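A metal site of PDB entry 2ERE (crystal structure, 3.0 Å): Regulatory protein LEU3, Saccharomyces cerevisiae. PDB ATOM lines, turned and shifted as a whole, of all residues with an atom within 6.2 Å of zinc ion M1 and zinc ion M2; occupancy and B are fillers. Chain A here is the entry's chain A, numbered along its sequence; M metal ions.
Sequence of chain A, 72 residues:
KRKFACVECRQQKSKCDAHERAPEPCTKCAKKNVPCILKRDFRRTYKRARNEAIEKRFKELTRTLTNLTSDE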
ATOM      1  N   ALA A   5      21.700  29.725  34.520  1.00  0.00           N
ATOM      2  CA  ALA A   5      22.333  29.818  33.200  1.00  0.00           C
ATOM      3  C   ALA A   5      23.512  28.865  33.003  1.00  0.00           C
ATOM      4  O   ALA A   5      24.319  28.632  33.919  1.00  0.00           O
ATOM      5  CB  ALA A   5      22.775  31.261  32.951  1.00  0.00           C
ATOM      6  N   CYS A   6      23.609  28.296  31.799  1.00  0.00           N
ATOM      7  CA  CYS A   6      24.685  27.375  31.492  1.00  0.00           C
ATOM      8  C   CYS A   6      25.967  28.166  31.314  1.00  0.00           C
ATOM      9  O   CYS A   6      25.945  29.328  30.938  1.00  0.00           O
ATOM     10  CB  CYS A   6      24.394  26.595  30.211  1.00  0.00           C
ATOM     11  SG  CYS A   6      24.422  27.566  28.718  1.00  0.00           S
ATOM     12  N   VAL A   7      27.090  27.514  31.576  1.00  0.00           N
ATOM     13  CA  VAL A   7      28.374  28.198  31.481  1.00  0.00           C
ATOM     14  C   VAL A   7      28.556  29.016  30.212  1.00  0.00           C
ATOM     15  O   VAL A   7      28.884  30.202  30.281  1.00  0.00           O
ATOM     16  CB  VAL A   7      29.531  27.211  31.573  1.00  0.00           C
ATOM     17  CG1 VAL A   7      30.817  27.955  31.838  1.00  0.00           C
ATOM     18  CG2 VAL A   7      29.260  26.231  32.682  1.00  0.00           C
ATOM     19  N   GLU A   8      28.339  28.396  29.058  1.00  0.00           N
ATOM     20  CA  GLU A   8      28.510  29.080  27.779  1.00  0.00           C
ATOM     21  C   GLU A   8      27.641  30.334  27.595  1.00  0.00           C
ATOM     22  O   GLU A   8      28.131  31.392  27.172  1.00  0.00           O
ATOM     23  CB  GLU A   8      28.257  28.086  26.633  1.00  0.00           C
ATOM     24  CG  GLU A   8      28.704  28.588  25.247  1.00  0.00           C
ATOM     25  CD  GLU A   8      30.188  28.944  25.203  1.00  0.00           C
ATOM     26  OE1 GLU A   8      30.979  28.302  25.937  1.00  0.00           O
ATOM     27  OE2 GLU A   8      30.561  29.851  24.416  1.00  0.00           O
ATOM     28  N   CYS A   9      26.349  30.203  27.906  1.00  0.00           N
ATOM     29  CA  CYS A   9      25.413  31.313  27.777  1.00  0.00           C
ATOM     30  C   CYS A   9      25.828  32.461  28.677  1.00  0.00           C
ATOM     31  O   CYS A   9      25.710  33.625  28.303  1.00  0.00           O
ATOM     32  CB  CYS A   9      23.996  30.867  28.128  1.00  0.00           C
ATOM     33  SG  CYS A   9      23.124  29.952  26.829  1.00  0.00           S
ATOM     34  N   ARG A  10      26.310  32.126  29.868  1.00  0.00           N
ATOM     35  CA  ARG A  10      26.765  33.122  30.824  1.00  0.00           C
ATOM     36  C   ARG A  10      27.892  33.907  30.211  1.00  0.00           C
ATOM     37  O   ARG A  10      28.002  35.119  30.403  1.00  0.00           O
ATOM     38  CB  ARG A  10      27.264  32.472  32.116  1.00  0.00           C
ATOM     39  CG  ARG A  10      26.171  32.046  33.042  1.00  0.00           C
ATOM     40  CD  ARG A  10      26.702  31.761  34.428  1.00  0.00           C
ATOM     41  NE  ARG A  10      25.614  31.579  35.378  1.00  0.00           N
ATOM     42  CZ  ARG A  10      25.789  31.205  36.640  1.00  0.00           C
ATOM     43  NH1 ARG A  10      27.007  30.984  37.085  1.00  0.00           N
ATOM     44  NH2 ARG A  10      24.741  31.040  37.435  1.00  0.00           N
ATOM     45  N   SER A  14      23.910  35.283  26.980  1.00  0.00           N
ATOM     46  CA  SER A  14      22.765  35.111  26.112  1.00  0.00           C
ATOM     47  C   SER A  14      21.639  34.417  26.867  1.00  0.00           C
ATOM     48  O   SER A  14      21.908  33.706  27.842  1.00  0.00           O
ATOM     49  CB  SER A  14      23.146  34.246  24.932  1.00  0.00           C
ATOM     50  OG  SER A  14      23.465  32.965  25.424  1.00  0.00           O
ATOM     51  N   LYS A  15      20.402  34.615  26.425  1.00  0.00           N
ATOM     52  CA  LYS A  15      19.270  33.960  27.075  1.00  0.00           C
ATOM     53  C   LYS A  15      19.590  32.472  27.002  1.00  0.00           C
ATOM     54  O   LYS A  15      19.976  31.984  25.947  1.00  0.00           O
ATOM     55  CB  LYS A  15      17.998  34.254  26.332  1.00  0.00           C
ATOM     56  N   CYS A  16      19.442  31.761  28.120  1.00  0.00           N
ATOM     57  CA  CYS A  16      19.719  30.318  28.170  1.00  0.00           C
ATOM     58  C   CYS A  16      18.482  29.514  28.548  1.00  0.00           C
ATOM     59  O   CYS A  16      17.823  29.831  29.541  1.00  0.00           O
ATOM     60  CB  CYS A  16      20.815  30.010  29.184  1.00  0.00           C
ATOM     61  SG  CYS A  16      21.095  28.247  29.446  1.00  0.00           S
ATOM     62  N   ASP A  17      18.162  28.483  27.753  1.00  0.00           N
ATOM     63  CA  ASP A  17      16.987  27.677  28.027  1.00  0.00           C
ATOM     64  C   ASP A  17      17.383  26.293  28.495  1.00  0.00           C
ATOM     65  O   ASP A  17      17.415  25.376  27.688  1.00  0.00           O
ATOM     66  CB  ASP A  17      16.116  27.571  26.792  1.00  0.00           C
ATOM     67  N   ALA A  18      17.683  26.150  29.785  1.00  0.00           N
ATOM     68  CA  ALA A  18      18.057  24.864  30.350  1.00  0.00           C
ATOM     69  C   ALA A  18      17.104  24.467  31.484  1.00  0.00           C
ATOM     70  O   ALA A  18      15.973  24.030  31.251  1.00  0.00           O
ATOM     71  CB  ALA A  18      19.502  24.915  30.859  1.00  0.00           C
ATOM     72  N   PRO A  25      21.168  19.587  27.187  1.00  0.00           N
ATOM     73  CA  PRO A  25      21.981  20.720  26.743  1.00  0.00           C
ATOM     74  C   PRO A  25      21.127  21.882  26.229  1.00  0.00           C
ATOM     75  O   PRO A  25      20.182  21.668  25.454  1.00  0.00           O
ATOM     76  CB  PRO A  25      22.849  20.098  25.646  1.00  0.00           C
ATOM     77  CG  PRO A  25      23.098  18.739  26.211  1.00  0.00           C
ATOM     78  CD  PRO A  25      21.718  18.312  26.700  1.00  0.00           C
ATOM     79  N   CYS A  26      21.447  23.096  26.674  1.00  0.00           N
ATOM     80  CA  CYS A  26      20.677  24.269  26.293  1.00  0.00           C
ATOM     81  C   CYS A  26      20.680  24.431  24.787  1.00  0.00           C
ATOM     82  O   CYS A  26      21.542  23.878  24.111  1.00  0.00           O
ATOM     83  CB  CYS A  26      21.224  25.527  26.959  1.00  0.00           C
ATOM     84  SG  CYS A  26      22.697  26.175  26.149  1.00  0.00           S
ATOM     85  N   THR A  27      19.719  25.199  24.284  1.00  0.00           N
ATOM     86  CA  THR A  27      19.569  25.437  22.835  1.00  0.00           C
ATOM     87  C   THR A  27      20.848  25.937  22.149  1.00  0.00           C
ATOM     88  O   THR A  27      21.376  25.304  21.241  1.00  0.00           O
ATOM     89  CB  THR A  27      18.452  26.465  22.588  1.00  0.00           C
ATOM     90  OG1 THR A  27      17.280  26.065  23.317  1.00  0.00           O
ATOM     91  CG2 THR A  27      18.146  26.552  21.085  1.00  0.00           C
ATOM     92  N   LYS A  28      21.329  27.095  22.587  1.00  0.00           N
ATOM     93  CA  LYS A  28      22.539  27.672  22.024  1.00  0.00           C
ATOM     94  C   LYS A  28      23.651  26.636  21.936  1.00  0.00           C
ATOM     95  O   LYS A  28      24.213  26.430  20.862  1.00  0.00           O
ATOM     96  CB  LYS A  28      22.990  28.851  22.872  1.00  0.00           C
ATOM     97  CG  LYS A  28      22.003  30.018  22.904  1.00  0.00           C
ATOM     98  CD  LYS A  28      21.732  30.607  21.515  1.00  0.00           C
ATOM     99  CE  LYS A  28      21.172  32.024  21.603  1.00  0.00           C
ATOM    100  NZ  LYS A  28      20.031  32.149  22.565  1.00  0.00           N
ATOM    101  N   CYS A  29      23.973  25.987  23.053  1.00  0.00           N
ATOM    102  CA  CYS A  29      25.026  24.965  23.075  1.00  0.00           C
ATOM    103  C   CYS A  29      24.776  23.882  22.034  1.00  0.00           C
ATOM    104  O   CYS A  29      25.605  22.992  21.849  1.00  0.00           O
ATOM    105  CB  CYS A  29      25.129  24.323  24.475  1.00  0.00           C
ATOM    106  SG  CYS A  29      25.994  25.301  25.728  1.00  0.00           S
ATOM    107  N   VAL A  34      28.477  21.902  22.060  1.00  0.00           N
ATOM    108  CA  VAL A  34      29.576  21.961  23.009  1.00  0.00           C
ATOM    109  C   VAL A  34      29.096  21.515  24.369  1.00  0.00           C
ATOM    110  O   VAL A  34      27.889  21.432  24.624  1.00  0.00           O
ATOM    111  CB  VAL A  34      30.137  23.390  23.131  1.00  0.00           C
ATOM    112  CG1 VAL A  34      30.558  23.898  21.759  1.00  0.00           C
ATOM    113  CG2 VAL A  34      29.086  24.290  23.745  1.00  0.00           C
ATOM    114  N   PRO A  35      30.039  21.202  25.254  1.00  0.00           N
ATOM    115  CA  PRO A  35      29.734  20.775  26.614  1.00  0.00           C
ATOM    116  C   PRO A  35      28.897  21.803  27.399  1.00  0.00           C
ATOM    117  O   PRO A  35      29.434  22.786  27.939  1.00  0.00           O
ATOM    118  CB  PRO A  35      31.117  20.563  27.208  1.00  0.00           C
ATOM    119  CG  PRO A  35      31.876  19.996  26.047  1.00  0.00           C
ATOM    120  CD  PRO A  35      31.401  20.793  24.851  1.00  0.00           C
ATOM    121  N   CYS A  36      27.593  21.568  27.482  1.00  0.00           N
ATOM    122  CA  CYS A  36      26.707  22.450  28.207  1.00  0.00           C
ATOM    123  C   CYS A  36      26.793  22.199  29.715  1.00  0.00           C
ATOM    124  O   CYS A  36      25.951  21.504  30.296  1.00  0.00           O
ATOM    125  CB  CYS A  36      25.282  22.249  27.745  1.00  0.00           C
ATOM    126  SG  CYS A  36      24.153  23.242  28.683  1.00  0.00           S
ATOM    127  N   ILE A  37      27.811  22.775  30.349  1.00  0.00           N
ATOM    128  CA  ILE A  37      27.996  22.609  31.777  1.00  0.00           C
ATOM    129  C   ILE A  37      27.062  23.521  32.566  1.00  0.00           C
ATOM    130  O   ILE A  37      26.613  24.561  32.076  1.00  0.00           O
ATOM    131  CB  ILE A  37      29.449  22.867  32.146  1.00  0.00           C
ATOM    132  N   LEU A  38      26.750  23.114  33.798  1.00  0.00           N
ATOM    133  CA  LEU A  38      25.903  23.883  34.684  1.00  0.00           C
ATOM    134  C   LEU A  38      26.724  24.119  35.944  1.00  0.00           C
ATOM    135  O   LEU A  38      26.560  23.392  36.912  1.00  0.00           O
ATOM    136  CB  LEU A  38      24.640  23.106  35.025  1.00  0.00           C
ATOM    137  CG  LEU A  38      23.515  23.060  33.996  1.00  0.00           C
ATOM    138  CD1 LEU A  38      22.760  24.366  34.005  1.00  0.00           C
ATOM    139  CD2 LEU A  38      24.076  22.759  32.620  1.00  0.00           C
HETATM  140 ZN    ZN M   1      22.458  27.980  27.697  1.00  0.00          ZN
HETATM  141 ZN    ZN M   2      24.231  25.383  27.417  1.00  0.00          ZN
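N of Val 34 sits at hydrogen-bond distance from O of Cys 29 (3.1 Å). The backbone carbonyl oxygen (O) of Cys 9 is in hydrogen-bond range of the backbone NH (N) of Ser 14 (2.8 Å).
Four residues have an atom within 4 Å of zinc ion M1: Cys 6, Cys 9, Cys 16 and Cys 26.
Of the 21 residues printed, 4 come within 4 Å of zinc ion M2. Along chain A the residues within 4 Å of zinc ion M2 span positions 6 to 36.
SG of Cys 16 is bound to zinc ion M1 (2.2 Å). SG of Cys 6 binds zinc ion M1. Zinc ion M1 is bound by the side-chain sulfur (SG) of Cys 9, at 2.3 Å. Zinc ion M1 is bound by SG of Cys 26, 2.4 Å away.
Zinc ion M2 is bound by SG of Cys 26 (2.1 Å), SG of Cys 29 (2.4 Å), SG of Cys 36 (2.5 Å) and SG of Cys 6 (2.5 Å).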
